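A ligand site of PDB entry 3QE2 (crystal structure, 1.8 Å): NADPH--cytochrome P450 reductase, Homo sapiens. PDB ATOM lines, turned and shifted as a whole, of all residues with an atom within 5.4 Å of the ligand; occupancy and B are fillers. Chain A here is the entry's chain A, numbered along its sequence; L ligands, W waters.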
ATOM      1  N   ARG A 239       3.689 -31.085  23.537  1.00  0.00           N
ATOM      2  CA  ARG A 239       4.716 -31.531  24.471  1.00  0.00           C
ATOM      3  C   ARG A 239       4.441 -30.851  25.806  1.00  0.00           C
ATOM      4  O   ARG A 239       3.729 -29.848  25.872  1.00  0.00           O
ATOM      5  CB  ARG A 239       6.107 -31.140  23.991  1.00  0.00           C
ATOM      6  CG  ARG A 239       6.513 -31.684  22.633  1.00  0.00           C
ATOM      7  CD  ARG A 239       8.024 -31.645  22.470  1.00  0.00           C
ATOM      8  NE  ARG A 239       8.569 -30.297  22.546  1.00  0.00           N
ATOM      9  CZ  ARG A 239       9.840 -30.020  22.816  1.00  0.00           C
ATOM     10  NH1 ARG A 239      10.698 -31.013  23.033  1.00  0.00           N
ATOM     11  NH2 ARG A 239      10.268 -28.765  22.859  1.00  0.00           N
ATOM     12  N   LEU A 241       6.489 -29.256  29.041  1.00  0.00           N
ATOM     13  CA  LEU A 241       7.741 -28.887  29.693  1.00  0.00           C
ATOM     14  C   LEU A 241       7.297 -28.244  30.989  1.00  0.00           C
ATOM     15  O   LEU A 241       6.363 -27.454  31.013  1.00  0.00           O
ATOM     16  CB  LEU A 241       8.546 -27.930  28.806  1.00  0.00           C
ATOM     17  CG  LEU A 241       9.193 -28.715  27.644  1.00  0.00           C
ATOM     18  CD1 LEU A 241       8.342 -28.559  26.394  1.00  0.00           C
ATOM     19  CD2 LEU A 241      10.628 -28.229  27.404  1.00  0.00           C
ATOM     20  N   VAL A 415      11.395 -31.936  30.529  1.00  0.00           N
ATOM     21  CA  VAL A 415      10.464 -32.180  29.435  1.00  0.00           C
ATOM     22  C   VAL A 415       9.887 -33.575  29.624  1.00  0.00           C
ATOM     23  O   VAL A 415      10.627 -34.534  29.859  1.00  0.00           O
ATOM     24  CB  VAL A 415      11.149 -32.062  28.040  1.00  0.00           C
ATOM     25  CG1 VAL A 415      12.366 -32.947  27.972  1.00  0.00           C
ATOM     26  CG2 VAL A 415      10.154 -32.427  26.938  1.00  0.00           C
ATOM     27  N   PRO A 474      20.478 -25.188  24.681  1.00  0.00           N
ATOM     28  CA  PRO A 474      19.185 -25.196  23.996  1.00  0.00           C
ATOM     29  C   PRO A 474      18.223 -26.200  24.649  1.00  0.00           C
ATOM     30  O   PRO A 474      18.659 -27.183  25.242  1.00  0.00           O
ATOM     31  CB  PRO A 474      19.552 -25.576  22.555  1.00  0.00           C
ATOM     32  CG  PRO A 474      20.793 -26.393  22.701  1.00  0.00           C
ATOM     33  CD  PRO A 474      21.549 -25.699  23.819  1.00  0.00           C
ATOM     34  N   GLY A 475      16.925 -25.936  24.557  1.00  0.00           N
ATOM     35  CA  GLY A 475      15.955 -26.827  25.178  1.00  0.00           C
ATOM     36  C   GLY A 475      16.109 -26.874  26.682  1.00  0.00           C
ATOM     37  O   GLY A 475      16.447 -25.871  27.315  1.00  0.00           O
ATOM     38  N   THR A 476      15.863 -28.040  27.281  1.00  0.00           N
ATOM     39  CA  THR A 476      15.999 -28.172  28.729  1.00  0.00           C
ATOM     40  C   THR A 476      17.449 -27.988  29.163  1.00  0.00           C
ATOM     41  O   THR A 476      17.766 -27.958  30.355  1.00  0.00           O
ATOM     42  CB  THR A 476      15.481 -29.537  29.201  1.00  0.00           C
ATOM     43  OG1 THR A 476      16.064 -30.577  28.400  1.00  0.00           O
ATOM     44  CG2 THR A 476      13.969 -29.585  29.099  1.00  0.00           C
ATOM     45  N   GLY A 477      18.339 -27.848  28.187  1.00  0.00           N
ATOM     46  CA  GLY A 477      19.735 -27.628  28.496  1.00  0.00           C
ATOM     47  C   GLY A 477      19.912 -26.259  29.143  1.00  0.00           C
ATOM     48  O   GLY A 477      20.976 -25.939  29.654  1.00  0.00           O
ATOM     49  N   GLY A 506      18.028 -22.029  22.708  1.00  0.00           N
ATOM     50  CA  GLY A 506      17.318 -22.360  21.487  1.00  0.00           C
ATOM     51  C   GLY A 506      16.106 -23.233  21.720  1.00  0.00           C
ATOM     52  O   GLY A 506      16.072 -24.042  22.648  1.00  0.00           O
ATOM     53  N   CYS A 507      15.096 -23.050  20.871  1.00  0.00           N
ATOM     54  CA  CYS A 507      13.872 -23.849  20.960  1.00  0.00           C
ATOM     55  C   CYS A 507      13.341 -23.984  19.537  1.00  0.00           C
ATOM     56  O   CYS A 507      13.889 -23.389  18.611  1.00  0.00           O
ATOM     57  CB  CYS A 507      12.839 -23.183  21.859  1.00  0.00           C
ATOM     58  SG  CYS A 507      12.332 -21.511  21.420  1.00  0.00           S
ATOM     59  N   ARG A 508      12.303 -24.783  19.361  1.00  0.00           N
ATOM     60  CA  ARG A 508      11.743 -24.984  18.025  1.00  0.00           C
ATOM     61  C   ARG A 508      11.014 -23.737  17.522  1.00  0.00           C
ATOM     62  O   ARG A 508      11.283 -23.261  16.413  1.00  0.00           O
ATOM     63  CB  ARG A 508      10.818 -26.203  18.037  1.00  0.00           C
ATOM     64  CG  ARG A 508      11.574 -27.462  18.458  1.00  0.00           C
ATOM     65  CD  ARG A 508      10.670 -28.649  18.690  1.00  0.00           C
ATOM     66  NE  ARG A 508      11.412 -29.742  19.310  1.00  0.00           N
ATOM     67  CZ  ARG A 508      10.933 -30.974  19.477  1.00  0.00           C
ATOM     68  NH1 ARG A 508       9.708 -31.261  19.057  1.00  0.00           N
ATOM     69  NH2 ARG A 508      11.672 -31.910  20.054  1.00  0.00           N
ATOM     70  N   ASP A 513       7.668 -23.459  22.497  1.00  0.00           N
ATOM     71  CA  ASP A 513       8.499 -24.028  23.550  1.00  0.00           C
ATOM     72  C   ASP A 513       9.663 -23.156  24.057  1.00  0.00           C
ATOM     73  O   ASP A 513      10.737 -23.667  24.352  1.00  0.00           O
ATOM     74  CB  ASP A 513       9.028 -25.387  23.090  1.00  0.00           C
ATOM     75  CG  ASP A 513       9.881 -25.299  21.833  1.00  0.00           C
ATOM     76  OD1 ASP A 513       9.799 -24.268  21.136  1.00  0.00           O
ATOM     77  OD2 ASP A 513      10.610 -26.262  21.534  1.00  0.00           O
ATOM     78  N   ALA A 535      18.099 -19.059  19.308  1.00  0.00           N
ATOM     79  CA  ALA A 535      17.966 -19.644  17.978  1.00  0.00           C
ATOM     80  C   ALA A 535      16.642 -20.405  17.874  1.00  0.00           C
ATOM     81  O   ALA A 535      16.429 -21.376  18.617  1.00  0.00           O
ATOM     82  CB  ALA A 535      19.132 -20.575  17.707  1.00  0.00           C
ATOM     83  N   SER A 537      14.831 -22.855  15.844  1.00  0.00           N
ATOM     84  CA  SER A 537      15.118 -23.858  14.825  1.00  0.00           C
ATOM     85  C   SER A 537      14.078 -24.139  13.752  1.00  0.00           C
ATOM     86  O   SER A 537      14.446 -24.468  12.622  1.00  0.00           O
ATOM     87  CB  SER A 537      15.480 -25.176  15.510  1.00  0.00           C
ATOM     88  OG  SER A 537      14.397 -25.654  16.282  1.00  0.00           O
ATOM     89  N   ARG A 538      12.798 -24.024  14.084  1.00  0.00           N
ATOM     90  CA  ARG A 538      11.757 -24.342  13.110  1.00  0.00           C
ATOM     91  C   ARG A 538      10.925 -23.180  12.590  1.00  0.00           C
ATOM     92  O   ARG A 538       9.792 -23.375  12.159  1.00  0.00           O
ATOM     93  CB  ARG A 538      10.851 -25.422  13.685  1.00  0.00           C
ATOM     94  CG  ARG A 538      11.622 -26.660  14.121  1.00  0.00           C
ATOM     95  CD  ARG A 538      10.722 -27.774  14.612  1.00  0.00           C
ATOM     96  NE  ARG A 538      11.514 -28.880  15.147  1.00  0.00           N
ATOM     97  CZ  ARG A 538      11.004 -30.052  15.526  1.00  0.00           C
ATOM     98  NH1 ARG A 538       9.702 -30.268  15.422  1.00  0.00           N
ATOM     99  NH2 ARG A 538      11.797 -30.993  16.010  1.00  0.00           N
ATOM    100  N   LYS A 543      17.415 -25.215   9.429  1.00  0.00           N
ATOM    101  CA  LYS A 543      17.622 -25.161  10.866  1.00  0.00           C
ATOM    102  C   LYS A 543      18.533 -24.014  11.273  1.00  0.00           C
ATOM    103  O   LYS A 543      19.536 -23.730  10.607  1.00  0.00           O
ATOM    104  CB  LYS A 543      18.267 -26.465  11.361  1.00  0.00           C
ATOM    105  CG  LYS A 543      17.445 -27.728  11.147  1.00  0.00           C
ATOM    106  CD  LYS A 543      16.198 -27.771  12.011  1.00  0.00           C
ATOM    107  CE  LYS A 543      15.548 -29.141  11.926  1.00  0.00           C
ATOM    108  NZ  LYS A 543      14.320 -29.267  12.750  1.00  0.00           N
ATOM    109  N   TYR A 545      20.426 -23.011  14.681  1.00  0.00           N
ATOM    110  CA  TYR A 545      20.821 -23.554  15.996  1.00  0.00           C
ATOM    111  C   TYR A 545      21.753 -22.618  16.772  1.00  0.00           C
ATOM    112  O   TYR A 545      22.268 -21.642  16.235  1.00  0.00           O
ATOM    113  CB  TYR A 545      21.537 -24.887  15.776  1.00  0.00           C
ATOM    114  CG  TYR A 545      20.662 -26.010  15.239  1.00  0.00           C
ATOM    115  CD1 TYR A 545      21.225 -27.045  14.484  1.00  0.00           C
ATOM    116  CD2 TYR A 545      19.308 -26.093  15.565  1.00  0.00           C
ATOM    117  CE1 TYR A 545      20.451 -28.134  14.063  1.00  0.00           C
ATOM    118  CE2 TYR A 545      18.532 -27.176  15.150  1.00  0.00           C
ATOM    119  CZ  TYR A 545      19.112 -28.196  14.404  1.00  0.00           C
ATOM    120  OH  TYR A 545      18.351 -29.279  14.028  1.00  0.00           O
ATOM    121  N   VAL A 546      21.991 -22.944  18.044  1.00  0.00           N
ATOM    122  CA  VAL A 546      22.879 -22.122  18.844  1.00  0.00           C
ATOM    123  C   VAL A 546      24.272 -21.962  18.212  1.00  0.00           C
ATOM    124  O   VAL A 546      24.850 -20.868  18.265  1.00  0.00           O
ATOM    125  CB  VAL A 546      23.023 -22.663  20.301  1.00  0.00           C
ATOM    126  CG1 VAL A 546      21.748 -22.394  21.082  1.00  0.00           C
ATOM    127  CG2 VAL A 546      23.330 -24.159  20.282  1.00  0.00           C
ATOM    128  N   GLN A 547      24.826 -23.028  17.623  1.00  0.00           N
ATOM    129  CA  GLN A 547      26.166 -22.904  17.036  1.00  0.00           C
ATOM    130  C   GLN A 547      26.225 -21.900  15.882  1.00  0.00           C
ATOM    131  O   GLN A 547      27.270 -21.318  15.607  1.00  0.00           O
ATOM    132  CB  GLN A 547      26.725 -24.270  16.582  1.00  0.00           C
ATOM    133  CG  GLN A 547      25.884 -25.066  15.579  1.00  0.00           C
ATOM    134  CD  GLN A 547      24.876 -25.973  16.259  1.00  0.00           C
ATOM    135  OE1 GLN A 547      24.526 -27.034  15.727  1.00  0.00           O
ATOM    136  NE2 GLN A 547      24.415 -25.574  17.425  1.00  0.00           N
ATOM    137  N   ASP A 572      21.615 -31.788  24.982  1.00  0.00           N
ATOM    138  CA  ASP A 572      21.858 -32.958  24.134  1.00  0.00           C
ATOM    139  C   ASP A 572      23.319 -33.285  23.863  1.00  0.00           C
ATOM    140  O   ASP A 572      24.056 -32.475  23.298  1.00  0.00           O
ATOM    141  CB  ASP A 572      21.135 -32.793  22.794  1.00  0.00           C
ATOM    142  CG  ASP A 572      21.468 -33.917  21.817  1.00  0.00           C
ATOM    143  OD1 ASP A 572      21.996 -33.630  20.720  1.00  0.00           O
ATOM    144  OD2 ASP A 572      21.193 -35.086  22.163  1.00  0.00           O
ATOM    145  N   ASN A 575      24.345 -34.886  19.532  1.00  0.00           N
ATOM    146  CA  ASN A 575      24.605 -34.014  18.397  1.00  0.00           C
ATOM    147  C   ASN A 575      24.954 -32.574  18.758  1.00  0.00           C
ATOM    148  O   ASN A 575      25.958 -32.053  18.284  1.00  0.00           O
ATOM    149  CB  ASN A 575      23.402 -34.051  17.464  1.00  0.00           C
ATOM    150  CG  ASN A 575      23.248 -35.398  16.790  1.00  0.00           C
ATOM    151  OD1 ASN A 575      22.155 -35.960  16.734  1.00  0.00           O
ATOM    152  ND2 ASN A 575      24.340 -35.936  16.270  1.00  0.00           N
ATOM    153  N   MET A 576      24.147 -31.940  19.596  1.00  0.00           N
ATOM    154  CA  MET A 576      24.383 -30.544  19.967  1.00  0.00           C
ATOM    155  C   MET A 576      25.777 -30.279  20.548  1.00  0.00           C
ATOM    156  O   MET A 576      26.490 -29.386  20.084  1.00  0.00           O
ATOM    157  CB  MET A 576      23.299 -30.063  20.932  1.00  0.00           C
ATOM    158  CG  MET A 576      23.368 -28.591  21.284  1.00  0.00           C
ATOM    159  SD  MET A 576      24.543 -28.200  22.592  1.00  0.00           S
ATOM    160  CE  MET A 576      23.693 -28.963  24.014  1.00  0.00           C
ATOM    161  N   ASP A 579      28.498 -30.534  17.806  1.00  0.00           N
ATOM    162  CA  ASP A 579      28.395 -29.442  16.838  1.00  0.00           C
ATOM    163  C   ASP A 579      28.878 -28.140  17.466  1.00  0.00           C
ATOM    164  O   ASP A 579      29.583 -27.358  16.824  1.00  0.00           O
ATOM    165  CB  ASP A 579      26.944 -29.278  16.357  1.00  0.00           C
ATOM    166  CG  ASP A 579      26.507 -30.411  15.435  1.00  0.00           C
ATOM    167  OD1 ASP A 579      25.284 -30.568  15.228  1.00  0.00           O
ATOM    168  OD2 ASP A 579      27.381 -31.128  14.913  1.00  0.00           O
HETATM  169  P1  LIG L   1      14.704 -30.175  21.959  1.00  0.00           P
HETATM  170  O1  LIG L   1      13.423 -29.462  21.708  1.00  0.00           O
HETATM  171  O2  LIG L   1      14.769 -31.550  21.383  1.00  0.00           O
HETATM  172  O3  LIG L   1      15.783 -29.368  21.340  1.00  0.00           O
HETATM  173  C1  LIG L   1      16.205 -28.056  21.762  1.00  0.00           C
HETATM  174  C2  LIG L   1      16.666 -27.230  20.569  1.00  0.00           C
HETATM  175  O4  LIG L   1      17.886 -27.860  20.081  1.00  0.00           O
HETATM  176  C3  LIG L   1      15.670 -27.254  19.397  1.00  0.00           C
HETATM  177  O5  LIG L   1      15.433 -25.938  18.847  1.00  0.00           O
HETATM  178  C4  LIG L   1      16.312 -28.198  18.416  1.00  0.00           C
HETATM  179  O6  LIG L   1      15.935 -28.021  17.039  1.00  0.00           O
HETATM  180  C5  LIG L   1      17.794 -27.913  18.681  1.00  0.00           C
HETATM  181  N1  LIG L   1      18.661 -28.856  18.150  1.00  0.00           N
HETATM  182  C6  LIG L   1      18.539 -30.156  17.623  1.00  0.00           C
HETATM  183  N2  LIG L   1      19.621 -30.858  17.149  1.00  0.00           N
HETATM  184  C7  LIG L   1      20.571 -29.877  17.399  1.00  0.00           C
HETATM  185  C8  LIG L   1      22.009 -29.851  17.156  1.00  0.00           C
HETATM  186  N3  LIG L   1      22.646 -30.867  16.599  1.00  0.00           N
HETATM  187  N4  LIG L   1      22.748 -28.775  17.484  1.00  0.00           N
HETATM  188  C9  LIG L   1      22.200 -27.652  18.061  1.00  0.00           C
HETATM  189  N5  LIG L   1      20.888 -27.515  18.341  1.00  0.00           N
HETATM  190  C10 LIG L   1      20.011 -28.670  18.004  1.00  0.00           C
HETATM  191  O7  LIG L   1      15.118 -30.091  23.398  1.00  0.00           O
HETATM  192  P2  LIG L   1      14.397 -30.855  24.560  1.00  0.00           P
HETATM  193  O8  LIG L   1      14.680 -32.274  24.159  1.00  0.00           O
HETATM  194  O9  LIG L   1      12.924 -30.707  24.542  1.00  0.00           O
HETATM  195  O10 LIG L   1      15.014 -30.456  25.865  1.00  0.00           O
HETATM  196  P3  LIG L   1      15.157 -29.137  16.142  1.00  0.00           P
HETATM  197  O11 LIG L   1      14.305 -30.104  17.109  1.00  0.00           O
HETATM  198  O12 LIG L   1      16.226 -29.967  15.310  1.00  0.00           O
HETATM  199  O13 LIG L   1      14.175 -28.324  15.205  1.00  0.00           O
HETATM  200  O   HOH W   1      17.462 -24.037  18.480  1.00  0.00           O
HETATM  201  O   HOH W   2      17.482 -32.525  21.236  1.00  0.00           O
HETATM  202  O   HOH W   3      21.667 -32.884  14.597  1.00  0.00           O
HETATM  203  O   HOH W   4      19.831 -31.870  19.968  1.00  0.00           O
HETATM  204  O   HOH W   5      15.082 -31.998  18.604  1.00  0.00           O
HETATM  205  O   HOH W   6      13.047 -26.808  22.165  1.00  0.00           O
HETATM  206  O   HOH W   7      19.364 -29.858  21.456  1.00  0.00           O
HETATM  207  O   HOH W   8      20.104 -24.787  19.190  1.00  0.00           O
HETATM  208  O   HOH W   9      19.831 -33.489  16.501  1.00  0.00           O
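The guanidinium group (NH2) of Arg 239 lies within salt-bridge range of the side-chain carboxylate (OD2) of Asp 513 (2.9 Å).
The backbone carbonyl oxygen (O) of Arg 508 is in hydrogen-bond range of the backbone NH (N) of Arg 538 (2.9 Å).
N of Ser 537 is in hydrogen-bond range of O of Cys 507, at 3.0 Å.
The side-chain sulfur (SG) of Cys 507 lies close to the side-chain carboxylate (OD1) of Asp 513, 3.8 Å away.
O of Ala 535 sits at hydrogen-bond distance from N of Cys 507.
OD1 of Asp 513 is in hydrogen-bond range of N of Arg 508 (3.1 Å).
The backbone NH of Asn 575 is in hydrogen-bond range of the side-chain carboxylate of Asp 572, at 2.9 Å.
N of Met 576 is in hydrogen-bond range of OD1 of Asp 572 (3.0 Å).
An oxygen (O12) of the ligand lies within hydrogen-bond range of the side-chain hydroxyl (OH) of Tyr 545 (2.6 Å).
NZ of Lys 543 lies within salt-bridge range of O13 of the ligand (2.6 Å).
The guanidinium group (NH1) of Arg 239 is in salt-bridge range of an oxygen (O9) of the ligand, 2.7 Å away.
NE of Arg 538 lies within salt-bridge range of O13 of the ligand, at 2.7 Å.
The backbone NH of Thr 476 lies within hydrogen-bond range of an oxygen (O10) of the ligand (2.9 Å).
The side-chain hydroxyl (OG1) of Thr 476 is in hydrogen-bond range of an oxygen (O10) of the ligand, at 2.7 Å.
The side-chain hydroxyl of Ser 537 lies within hydrogen-bond range of an oxygen (O5) of the ligand, at 2.8 Å.
An oxygen (O5) of the ligand sits close to the backbone carbonyl oxygen of Cys 507 (3.0 Å).
The side-chain carboxylate (OD1) of Asp 579 sits at hydrogen-bond distance from a nitrogen (N3) of the ligand.
The side-chain amide oxygen (OE1) of Gln 547 sits close to a nitrogen (N4) of the ligand, at 3.0 Å.
The backbone NH (N) of Arg 508 lies within hydrogen-bond range of an oxygen (O5) of the ligand (3.4 Å).
An oxygen (O1) of the ligand lies within salt-bridge range of the guanidinium group (NE) of Arg 508.
Merely in contact with the ligand: Asn 575, Met 576, Gly 475, Pro 474 and Gly 506.
Hydrophobic or aromatic side chains that line the ligand: Pro 474, Tyr 545 and Met 576.
Along chain A the residues within 4 Å of the ligand span positions 239 to 579.
Water W9 lies within hydrogen-bond range of N2 of the ligand (2.7 Å) and OD1 of Asn 575 (3.4 Å).
Water W6 lies within hydrogen-bond range of the side-chain carboxylate of Asp 513 (2.6 Å), an oxygen (O1) of the ligand (2.7 Å) and the guanidinium group of Arg 239 (3.5 Å).
Water W1 bridges O5 of the ligand and O of Ala 535.
Water W8 bridges the backbone NH (N) of Val 546 and a nitrogen (N5) of the ligand.
Water W4 bridges OD1 of Asp 572 and N2 of the ligand.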
